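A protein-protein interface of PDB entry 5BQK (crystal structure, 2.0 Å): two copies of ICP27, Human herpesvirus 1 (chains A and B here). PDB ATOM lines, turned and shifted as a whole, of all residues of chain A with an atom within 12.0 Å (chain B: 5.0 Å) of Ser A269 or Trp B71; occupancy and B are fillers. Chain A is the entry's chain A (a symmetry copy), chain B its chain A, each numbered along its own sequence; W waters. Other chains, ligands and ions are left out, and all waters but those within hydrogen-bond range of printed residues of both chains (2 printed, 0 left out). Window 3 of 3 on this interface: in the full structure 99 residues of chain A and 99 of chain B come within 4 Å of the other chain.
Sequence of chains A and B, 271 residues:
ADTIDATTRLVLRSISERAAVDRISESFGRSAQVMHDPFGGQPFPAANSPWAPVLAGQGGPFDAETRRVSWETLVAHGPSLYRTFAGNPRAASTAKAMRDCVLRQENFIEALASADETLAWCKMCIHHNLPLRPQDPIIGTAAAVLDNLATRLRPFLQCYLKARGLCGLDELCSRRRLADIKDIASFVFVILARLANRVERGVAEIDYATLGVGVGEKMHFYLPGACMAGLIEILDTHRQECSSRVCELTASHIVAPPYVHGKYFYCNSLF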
ATOM      1  N   LEU A  12       1.494  12.684  29.423  1.00  0.00           N
ATOM      2  CA  LEU A  12       2.264  13.238  28.276  1.00  0.00           C
ATOM      3  C   LEU A  12       2.946  14.570  28.579  1.00  0.00           C
ATOM      4  O   LEU A  12       4.149  14.734  28.313  1.00  0.00           O
ATOM      5  CB  LEU A  12       1.371  13.349  27.033  1.00  0.00           C
ATOM      6  CG  LEU A  12       0.803  12.026  26.531  1.00  0.00           C
ATOM      7  CD1 LEU A  12       0.005  12.271  25.233  1.00  0.00           C
ATOM      8  CD2 LEU A  12       1.983  11.067  26.230  1.00  0.00           C
ATOM      9  N   ARG A  13       2.200  15.523  29.154  1.00  0.00           N
ATOM     10  CA  ARG A  13       2.836  16.773  29.525  1.00  0.00           C
ATOM     11  C   ARG A  13       3.907  16.634  30.634  1.00  0.00           C
ATOM     12  O   ARG A  13       4.838  17.434  30.701  1.00  0.00           O
ATOM     13  CB  ARG A  13       1.826  17.868  29.860  1.00  0.00           C
ATOM     14  CG  ARG A  13       0.754  18.066  28.763  1.00  0.00           C
ATOM     15  CD  ARG A  13      -0.515  18.754  29.327  1.00  0.00           C
ATOM     16  NE  ARG A  13      -0.070  19.779  30.257  1.00  0.00           N
ATOM     17  CZ  ARG A  13      -0.453  19.893  31.544  1.00  0.00           C
ATOM     18  NH1 ARG A  13       0.080  20.856  32.283  1.00  0.00           N
ATOM     19  NH2 ARG A  13      -1.386  19.089  32.094  1.00  0.00           N
ATOM     20  N   SER A  14       3.830  15.591  31.452  1.00  0.00           N
ATOM     21  CA  SER A  14       4.712  15.574  32.649  1.00  0.00           C
ATOM     22  C   SER A  14       6.180  15.236  32.282  1.00  0.00           C
ATOM     23  O   SER A  14       7.063  15.273  33.127  1.00  0.00           O
ATOM     24  CB  SER A  14       4.177  14.579  33.685  1.00  0.00           C
ATOM     25  OG  SER A  14       4.551  13.239  33.302  1.00  0.00           O
ATOM     26  N   ILE A  15       6.445  14.882  31.020  1.00  0.00           N
ATOM     27  CA  ILE A  15       7.823  14.641  30.577  1.00  0.00           C
ATOM     28  C   ILE A  15       8.613  15.968  30.794  1.00  0.00           C
ATOM     29  O   ILE A  15       9.783  15.978  31.178  1.00  0.00           O
ATOM     30  CB  ILE A  15       7.798  14.256  29.095  1.00  0.00           C
ATOM     31  CG1 ILE A  15       9.205  14.027  28.539  1.00  0.00           C
ATOM     32  CG2 ILE A  15       7.170  15.416  28.311  1.00  0.00           C
ATOM     33  CD1 ILE A  15       9.940  12.843  29.247  1.00  0.00           C
ATOM     34  N   SER A  16       7.936  17.085  30.582  1.00  0.00           N
ATOM     35  CA  SER A  16       8.502  18.394  30.778  1.00  0.00           C
ATOM     36  C   SER A  16       8.995  18.596  32.215  1.00  0.00           C
ATOM     37  O   SER A  16       9.857  19.405  32.471  1.00  0.00           O
ATOM     38  CB  SER A  16       7.418  19.410  30.533  1.00  0.00           C
ATOM     39  OG  SER A  16       7.771  20.630  31.118  1.00  0.00           O
ATOM     40  N   GLU A  17       8.434  17.852  33.160  1.00  0.00           N
ATOM     41  CA  GLU A  17       8.813  18.100  34.523  1.00  0.00           C
ATOM     42  C   GLU A  17      10.139  17.352  34.764  1.00  0.00           C
ATOM     43  O   GLU A  17      10.997  17.817  35.554  1.00  0.00           O
ATOM     44  CB  GLU A  17       7.629  17.799  35.457  1.00  0.00           C
ATOM     45  CG  GLU A  17       7.845  16.917  36.665  1.00  0.00           C
ATOM     46  CD  GLU A  17       6.526  16.197  37.017  1.00  0.00           C
ATOM     47  OE1 GLU A  17       5.540  16.917  37.241  1.00  0.00           O
ATOM     48  OE2 GLU A  17       6.459  14.924  36.991  1.00  0.00           O
ATOM     49  N   ARG A  18      10.384  16.288  34.000  1.00  0.00           N
ATOM     50  CA  ARG A  18      11.628  15.514  34.245  1.00  0.00           C
ATOM     51  C   ARG A  18      12.773  15.664  33.222  1.00  0.00           C
ATOM     52  O   ARG A  18      13.929  15.339  33.543  1.00  0.00           O
ATOM     53  CB  ARG A  18      11.320  14.021  34.527  1.00  0.00           C
ATOM     54  CG  ARG A  18      10.073  13.731  35.481  1.00  0.00           C
ATOM     55  CD  ARG A  18       9.675  12.198  35.503  1.00  0.00           C
ATOM     56  NE  ARG A  18       9.315  11.675  34.180  1.00  0.00           N
ATOM     57  CZ  ARG A  18       8.107  11.770  33.589  1.00  0.00           C
ATOM     58  NH1 ARG A  18       7.923  11.274  32.358  1.00  0.00           N
ATOM     59  NH2 ARG A  18       7.078  12.365  34.185  1.00  0.00           N
ATOM     60  N   ALA A  19      12.489  16.128  31.994  1.00  0.00           N
ATOM     61  CA  ALA A  19      13.501  16.028  30.947  1.00  0.00           C
ATOM     62  C   ALA A  19      14.585  17.091  31.136  1.00  0.00           C
ATOM     63  O   ALA A  19      14.275  18.267  31.282  1.00  0.00           O
ATOM     64  CB  ALA A  19      12.878  16.131  29.583  1.00  0.00           C
ATOM     65  N   ALA A  20      15.853  16.694  31.105  1.00  0.00           N
ATOM     66  CA  ALA A  20      16.926  17.654  31.369  1.00  0.00           C
ATOM     67  C   ALA A  20      18.236  17.157  30.817  1.00  0.00           C
ATOM     68  O   ALA A  20      18.487  15.934  30.770  1.00  0.00           O
ATOM     69  CB  ALA A  20      17.067  17.955  32.897  1.00  0.00           C
ATOM     70  N   VAL A  21      19.079  18.084  30.404  1.00  0.00           N
ATOM     71  CA  VAL A  21      20.330  17.673  29.711  1.00  0.00           C
ATOM     72  C   VAL A  21      21.118  16.695  30.536  1.00  0.00           C
ATOM     73  O   VAL A  21      21.627  15.705  30.012  1.00  0.00           O
ATOM     74  CB  VAL A  21      21.209  18.857  29.294  1.00  0.00           C
ATOM     75  CG1 VAL A  21      22.670  18.377  28.943  1.00  0.00           C
ATOM     76  CG2 VAL A  21      20.574  19.570  28.105  1.00  0.00           C
ATOM     77  N   ILE A  24      19.503  13.109  30.694  1.00  0.00           N
ATOM     78  CA  ILE A  24      19.843  12.469  29.418  1.00  0.00           C
ATOM     79  C   ILE A  24      21.306  11.979  29.387  1.00  0.00           C
ATOM     80  O   ILE A  24      21.589  10.858  28.932  1.00  0.00           O
ATOM     81  CB  ILE A  24      19.610  13.419  28.186  1.00  0.00           C
ATOM     82  CG1 ILE A  24      18.161  13.978  28.106  1.00  0.00           C
ATOM     83  CG2 ILE A  24      20.032  12.718  26.908  1.00  0.00           C
ATOM     84  CD1 ILE A  24      17.095  12.941  27.921  1.00  0.00           C
ATOM     85  N   PHE A 265      14.371  21.282  10.410  1.00  0.00           N
ATOM     86  CA  PHE A 265      14.568  21.973  11.702  1.00  0.00           C
ATOM     87  C   PHE A 265      14.624  20.960  12.814  1.00  0.00           C
ATOM     88  O   PHE A 265      14.280  19.762  12.629  1.00  0.00           O
ATOM     89  CB  PHE A 265      13.505  23.081  11.915  1.00  0.00           C
ATOM     90  CG  PHE A 265      12.089  22.557  12.099  1.00  0.00           C
ATOM     91  CD1 PHE A 265      11.678  21.995  13.349  1.00  0.00           C
ATOM     92  CD2 PHE A 265      11.177  22.622  11.050  1.00  0.00           C
ATOM     93  CE1 PHE A 265      10.341  21.516  13.512  1.00  0.00           C
ATOM     94  CE2 PHE A 265       9.823  22.145  11.176  1.00  0.00           C
ATOM     95  CZ  PHE A 265       9.405  21.596  12.407  1.00  0.00           C
ATOM     96  N   TYR A 266      15.106  21.413  13.955  1.00  0.00           N
ATOM     97  CA  TYR A 266      15.135  20.620  15.157  1.00  0.00           C
ATOM     98  C   TYR A 266      14.436  21.520  16.166  1.00  0.00           C
ATOM     99  O   TYR A 266      14.831  22.696  16.307  1.00  0.00           O
ATOM    100  CB  TYR A 266      16.602  20.295  15.547  1.00  0.00           C
ATOM    101  CG  TYR A 266      16.781  19.745  16.978  1.00  0.00           C
ATOM    102  CD1 TYR A 266      16.093  18.608  17.401  1.00  0.00           C
ATOM    103  CD2 TYR A 266      17.633  20.366  17.892  1.00  0.00           C
ATOM    104  CE1 TYR A 266      16.239  18.073  18.683  1.00  0.00           C
ATOM    105  CE2 TYR A 266      17.817  19.833  19.202  1.00  0.00           C
ATOM    106  CZ  TYR A 266      17.096  18.672  19.582  1.00  0.00           C
ATOM    107  OH  TYR A 266      17.233  18.086  20.828  1.00  0.00           O
ATOM    108  N   CYS A 267      13.391  21.000  16.846  1.00  0.00           N
ATOM    109  CA  CYS A 267      12.613  21.784  17.850  1.00  0.00           C
ATOM    110  C   CYS A 267      12.435  20.893  19.097  1.00  0.00           C
ATOM    111  O   CYS A 267      11.850  19.768  19.070  1.00  0.00           O
ATOM    112  CB  CYS A 267      11.270  22.283  17.289  1.00  0.00           C
ATOM    113  SG  CYS A 267      10.290  23.411  18.327  1.00  0.00           S
ATOM    114  N   ASN A 268      13.033  21.364  20.195  1.00  0.00           N
ATOM    115  CA  ASN A 268      12.984  20.606  21.422  1.00  0.00           C
ATOM    116  C   ASN A 268      12.862  21.634  22.557  1.00  0.00           C
ATOM    117  O   ASN A 268      13.819  22.370  22.858  1.00  0.00           O
ATOM    118  CB  ASN A 268      14.246  19.760  21.554  1.00  0.00           C
ATOM    119  CG  ASN A 268      14.268  18.972  22.853  1.00  0.00           C
ATOM    120  OD1 ASN A 268      13.485  19.254  23.798  1.00  0.00           O
ATOM    121  ND2 ASN A 268      15.187  18.007  22.934  1.00  0.00           N
ATOM    122  N   SER A 269      11.657  21.702  23.103  1.00  0.00           N
ATOM    123  CA  SER A 269      11.220  22.701  24.064  1.00  0.00           C
ATOM    124  C   SER A 269      11.557  22.280  25.485  1.00  0.00           C
ATOM    125  O   SER A 269      11.315  23.042  26.435  1.00  0.00           O
ATOM    126  CB  SER A 269       9.679  22.826  23.982  1.00  0.00           C
ATOM    127  OG  SER A 269       9.298  23.640  22.887  1.00  0.00           O
ATOM    128  N   LEU A 270      12.014  21.055  25.652  1.00  0.00           N
ATOM    129  CA  LEU A 270      12.061  20.449  27.001  1.00  0.00           C
ATOM    130  C   LEU A 270      13.451  20.494  27.556  1.00  0.00           C
ATOM    131  O   LEU A 270      13.635  20.426  28.776  1.00  0.00           O
ATOM    132  CB  LEU A 270      11.636  18.964  26.963  1.00  0.00           C
ATOM    133  CG  LEU A 270      10.242  18.765  26.346  1.00  0.00           C
ATOM    134  CD1 LEU A 270       9.859  17.340  26.399  1.00  0.00           C
ATOM    135  CD2 LEU A 270       9.197  19.607  27.101  1.00  0.00           C
ATOM    136  N   PHE A 271      14.424  20.454  26.654  1.00  0.00           N
ATOM    137  CA  PHE A 271      15.811  20.538  27.043  1.00  0.00           C
ATOM    138  C   PHE A 271      16.754  20.959  25.909  1.00  0.00           C
ATOM    139  O   PHE A 271      17.899  21.307  26.255  1.00  0.00           O
ATOM    140  CB  PHE A 271      16.302  19.247  27.717  1.00  0.00           C
ATOM    141  CG  PHE A 271      16.494  18.071  26.764  1.00  0.00           C
ATOM    142  CD1 PHE A 271      17.718  17.864  26.106  1.00  0.00           C
ATOM    143  CD2 PHE A 271      15.476  17.151  26.552  1.00  0.00           C
ATOM    144  CE1 PHE A 271      17.911  16.793  25.256  1.00  0.00           C
ATOM    145  CE2 PHE A 271      15.662  16.058  25.696  1.00  0.00           C
ATOM    146  CZ  PHE A 271      16.889  15.890  25.036  1.00  0.00           C
ATOM    147  N   VAL B  69      15.318  25.480  16.147  1.00  0.00           N
ATOM    148  CA  VAL B  69      14.364  26.570  16.299  1.00  0.00           C
ATOM    149  C   VAL B  69      13.613  26.380  17.625  1.00  0.00           C
ATOM    150  O   VAL B  69      13.306  25.212  18.067  1.00  0.00           O
ATOM    151  CB  VAL B  69      13.331  26.654  15.070  1.00  0.00           C
ATOM    152  CG1 VAL B  69      14.043  26.956  13.698  1.00  0.00           C
ATOM    153  CG2 VAL B  69      12.411  25.388  14.961  1.00  0.00           C
ATOM    154  N   SER B  70      13.287  27.489  18.292  1.00  0.00           N
ATOM    155  CA  SER B  70      12.366  27.412  19.477  1.00  0.00           C
ATOM    156  C   SER B  70      10.945  27.125  18.954  1.00  0.00           C
ATOM    157  O   SER B  70      10.681  27.361  17.763  1.00  0.00           O
ATOM    158  CB  SER B  70      12.320  28.744  20.184  1.00  0.00           C
ATOM    159  OG  SER B  70      11.745  29.628  19.249  1.00  0.00           O
ATOM    160  N   TRP B  71      10.053  26.618  19.794  1.00  0.00           N
ATOM    161  CA  TRP B  71       8.611  26.524  19.429  1.00  0.00           C
ATOM    162  C   TRP B  71       8.095  27.877  18.918  1.00  0.00           C
ATOM    163  O   TRP B  71       7.367  27.988  17.899  1.00  0.00           O
ATOM    164  CB  TRP B  71       7.768  26.035  20.632  1.00  0.00           C
ATOM    165  CG  TRP B  71       6.256  26.128  20.359  1.00  0.00           C
ATOM    166  CD1 TRP B  71       5.374  26.879  21.048  1.00  0.00           C
ATOM    167  CD2 TRP B  71       5.468  25.466  19.285  1.00  0.00           C
ATOM    168  NE1 TRP B  71       4.089  26.767  20.497  1.00  0.00           N
ATOM    169  CE2 TRP B  71       4.126  25.895  19.429  1.00  0.00           C
ATOM    170  CE3 TRP B  71       5.771  24.559  18.266  1.00  0.00           C
ATOM    171  CZ2 TRP B  71       3.077  25.448  18.570  1.00  0.00           C
ATOM    172  CZ3 TRP B  71       4.722  24.087  17.404  1.00  0.00           C
ATOM    173  CH2 TRP B  71       3.413  24.558  17.549  1.00  0.00           C
ATOM    174  N   GLU B  72       8.458  28.944  19.605  1.00  0.00           N
ATOM    175  CA  GLU B  72       8.012  30.269  19.185  1.00  0.00           C
ATOM    176  C   GLU B  72       8.541  30.698  17.810  1.00  0.00           C
ATOM    177  O   GLU B  72       7.853  31.348  17.025  1.00  0.00           O
ATOM    178  CB  GLU B  72       8.331  31.306  20.273  1.00  0.00           C
ATOM    179  CG  GLU B  72       8.083  30.753  21.756  1.00  0.00           C
ATOM    180  CD  GLU B  72       9.238  29.668  22.201  1.00  0.00           C
ATOM    181  N   THR B  73       9.769  30.360  17.501  1.00  0.00           N
ATOM    182  CA  THR B  73      10.305  30.601  16.157  1.00  0.00           C
ATOM    183  C   THR B  73       9.572  29.796  15.064  1.00  0.00           C
ATOM    184  O   THR B  73       9.327  30.315  13.934  1.00  0.00           O
ATOM    185  CB  THR B  73      11.834  30.275  16.102  1.00  0.00           C
ATOM    186  OG1 THR B  73      12.500  31.224  16.932  1.00  0.00           O
ATOM    187  CG2 THR B  73      12.419  30.444  14.677  1.00  0.00           C
ATOM    188  N   LEU B  74       9.291  28.521  15.358  1.00  0.00           N
ATOM    189  CA  LEU B  74       8.525  27.652  14.409  1.00  0.00           C
ATOM    190  C   LEU B  74       7.128  28.268  14.106  1.00  0.00           C
ATOM    191  O   LEU B  74       6.710  28.389  12.932  1.00  0.00           O
ATOM    192  CB  LEU B  74       8.413  26.207  14.966  1.00  0.00           C
ATOM    193  CG  LEU B  74       7.685  25.197  14.090  1.00  0.00           C
ATOM    194  CD1 LEU B  74       8.394  25.033  12.674  1.00  0.00           C
ATOM    195  CD2 LEU B  74       7.524  23.889  14.858  1.00  0.00           C
ATOM    196  N   VAL B  75       6.461  28.774  15.151  1.00  0.00           N
ATOM    197  CA  VAL B  75       5.166  29.435  14.949  1.00  0.00           C
ATOM    198  C   VAL B  75       5.320  30.744  14.148  1.00  0.00           C
ATOM    199  O   VAL B  75       4.439  31.159  13.367  1.00  0.00           O
ATOM    200  CB  VAL B  75       4.540  29.801  16.300  1.00  0.00           C
ATOM    201  CG1 VAL B  75       3.355  30.802  16.094  1.00  0.00           C
ATOM    202  CG2 VAL B  75       4.137  28.533  17.138  1.00  0.00           C
ATOM    203  N   ALA B 120       5.771  18.572  15.789  1.00  0.00           N
ATOM    204  CA  ALA B 120       5.809  20.023  15.995  1.00  0.00           C
ATOM    205  C   ALA B 120       5.310  20.769  14.748  1.00  0.00           C
ATOM    206  O   ALA B 120       4.627  21.833  14.799  1.00  0.00           O
ATOM    207  CB  ALA B 120       7.277  20.434  16.335  1.00  0.00           C
ATOM    208  N   LYS B 123       1.518  20.553  14.794  1.00  0.00           N
ATOM    209  CA  LYS B 123       1.071  21.485  15.837  1.00  0.00           C
ATOM    210  C   LYS B 123       1.149  22.898  15.360  1.00  0.00           C
ATOM    211  O   LYS B 123       0.216  23.685  15.602  1.00  0.00           O
ATOM    212  CB  LYS B 123       1.917  21.361  17.115  1.00  0.00           C
ATOM    213  CG  LYS B 123       1.218  22.073  18.334  1.00  0.00           C
ATOM    214  CD  LYS B 123       1.989  21.862  19.659  1.00  0.00           C
ATOM    215  CE  LYS B 123       1.311  22.673  20.829  1.00  0.00           C
ATOM    216  NZ  LYS B 123       1.946  22.220  22.148  1.00  0.00           N
ATOM    217  N   MET B 124       2.223  23.254  14.681  1.00  0.00           N
ATOM    218  CA  MET B 124       2.280  24.612  14.071  1.00  0.00           C
ATOM    219  C   MET B 124       1.169  24.835  13.031  1.00  0.00           C
ATOM    220  O   MET B 124       0.573  25.939  12.981  1.00  0.00           O
ATOM    221  CB  MET B 124       3.633  24.877  13.420  1.00  0.00           C
ATOM    222  CG  MET B 124       3.737  26.260  12.823  1.00  0.00           C
ATOM    223  SD  MET B 124       3.160  26.350  10.956  1.00  0.00           S
ATOM    224  CE  MET B 124       4.320  25.016  10.167  1.00  0.00           C
ATOM    225  N   HIS B 127      -1.946  25.300  14.854  1.00  0.00           N
ATOM    226  CA  HIS B 127      -1.930  26.628  15.443  1.00  0.00           C
ATOM    227  C   HIS B 127      -2.405  27.633  14.424  1.00  0.00           C
ATOM    228  O   HIS B 127      -3.138  28.555  14.771  1.00  0.00           O
ATOM    229  CB  HIS B 127      -0.542  26.996  15.961  1.00  0.00           C
ATOM    230  CG  HIS B 127      -0.428  28.413  16.439  1.00  0.00           C
ATOM    231  ND1 HIS B 127      -0.494  28.765  17.775  1.00  0.00           N
ATOM    232  CD2 HIS B 127      -0.221  29.570  15.760  1.00  0.00           C
ATOM    233  CE1 HIS B 127      -0.323  30.077  17.901  1.00  0.00           C
ATOM    234  NE2 HIS B 127      -0.174  30.588  16.694  1.00  0.00           N
ATOM    235  N   PRO B 224       6.951  19.986  21.930  1.00  0.00           N
ATOM    236  CA  PRO B 224       8.054  19.646  21.028  1.00  0.00           C
ATOM    237  C   PRO B 224       9.248  19.119  21.801  1.00  0.00           C
ATOM    238  O   PRO B 224       9.713  19.758  22.752  1.00  0.00           O
ATOM    239  CB  PRO B 224       8.351  20.983  20.352  1.00  0.00           C
ATOM    240  CG  PRO B 224       6.915  21.593  20.278  1.00  0.00           C
ATOM    241  CD  PRO B 224       6.473  21.372  21.669  1.00  0.00           C
ATOM    242  N   GLY B 225       9.682  17.928  21.450  1.00  0.00           N
ATOM    243  CA  GLY B 225      10.821  17.290  22.125  1.00  0.00           C
ATOM    244  C   GLY B 225      10.325  16.093  22.938  1.00  0.00           C
ATOM    245  O   GLY B 225      11.122  15.292  23.380  1.00  0.00           O
HETATM  246  O   HOH W   1      14.270  23.910  20.237  1.00  0.00           O
HETATM  247  O   HOH W   2      10.778  26.039  22.301  1.00  0.00           O
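Along chain A the printed residues that touch a printed residue of chain B span positions 265 to 270. Hydrophobic or aromatic side chains of chain B that line the printed part of chain A: Val B69, Trp B71, Leu B74 and Pro B224.
No position is printed for both chains.
Ser A269 touches two residues of chain B. Of the printed residues of chain A, Trp B71 touches Cys A267 and Ser A269. Of the printed residues of chain A, Ser B70 touches Cys A267. Leu B74 touches just one residue of chain A: Phe A265 (3.6 Å). No residue of chain A comes within 4 Å of Lys B123. His B127 touches none of the printed residues of chain A. Printed residues of chain A within 4 Å of Gly B225: Cys A267, Asn A268 and Leu A270. Printed residues of chain B within 4 Å of Tyr A266: Val B69 (2.8 Å). Of the printed residues of chain B, Leu A270 touches Pro B224 (3.8 Å) and Gly B225 (3.7 Å). Printed residues of chain B within 4 Å of Phe A265: Val B69 (3.8 Å) and Leu B74 (3.6 Å). Of the printed residues of chain B, Cys A267 touches Val B69, Ser B70, Trp B71, Pro B224 and Gly B225. Printed residues of chain B within 4 Å of Asn A268: Pro B224 (3.6 Å) and Gly B225 (3.7 Å). Arg A18 touches none of the printed residues of chain B. Glu A17 touches none of the printed residues of chain B. The nearest printed residue of chain B that does not touch Leu A270 is Trp B71 (8.2 Å).
The backbone carbonyl oxygen (O) of Tyr A266 lies within hydrogen-bond range of the backbone NH (N) of Val B69, at 2.8 Å. The side-chain sulfur (SG) of Cys A267 lies close to the backbone carbonyl oxygen (O) of Val B69 (3.5 Å). The backbone NH of Trp B71 is in hydrogen-bond range of the side-chain sulfur of Cys A267, at 3.5 Å. The backbone carbonyl oxygen (O) of Pro B224 is in hydrogen-bond range of the backbone NH (N) of Ser A269 (2.8 Å).
Water W2 bridges the backbone NH (N) of Trp B71 (2.7 Å) and the side-chain hydroxyl (OG) of Ser A269 (2.9 Å). Water W1 lies within hydrogen-bond range of O of Val B69 (2.7 Å) and N of Asn A268 (2.8 Å).
The backbone NH (N) of Glu B72 lies close to the side-chain hydroxyl (OG) of Ser B70 (3.4 Å). The backbone NH (N) of Thr B73 lies within hydrogen-bond range of the side-chain hydroxyl (OG) of Ser B70 (2.7 Å). The side-chain hydroxyl (OH) of Tyr A266 is in hydrogen-bond range of the side-chain amide nitrogen (ND2) of Asn A268 (2.9 Å). N of Leu A270 is in hydrogen-bond range of OD1 of Asn A268 (3.0 Å). OD1 of Asn A268 is in hydrogen-bond range of N of Phe A271.
Among the printed residues, merely in contact across the chains: Phe A265 with Val B69 (3.8 Å), Phe A265 with Leu B74 (3.6 Å), Cys A267 with Ser B70 (3.8 Å), Cys A267 with Pro B224 (3.7 Å), Cys A267 with Gly B225 (3.7 Å), Asn A268 with Pro B224 (3.6 Å), Asn A268 with Gly B225 (3.7 Å), Ser A269 with Trp B71 (3.6 Å), Leu A270 with Pro B224 (3.8 Å) and Leu A270 with Gly B225 (3.7 Å).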
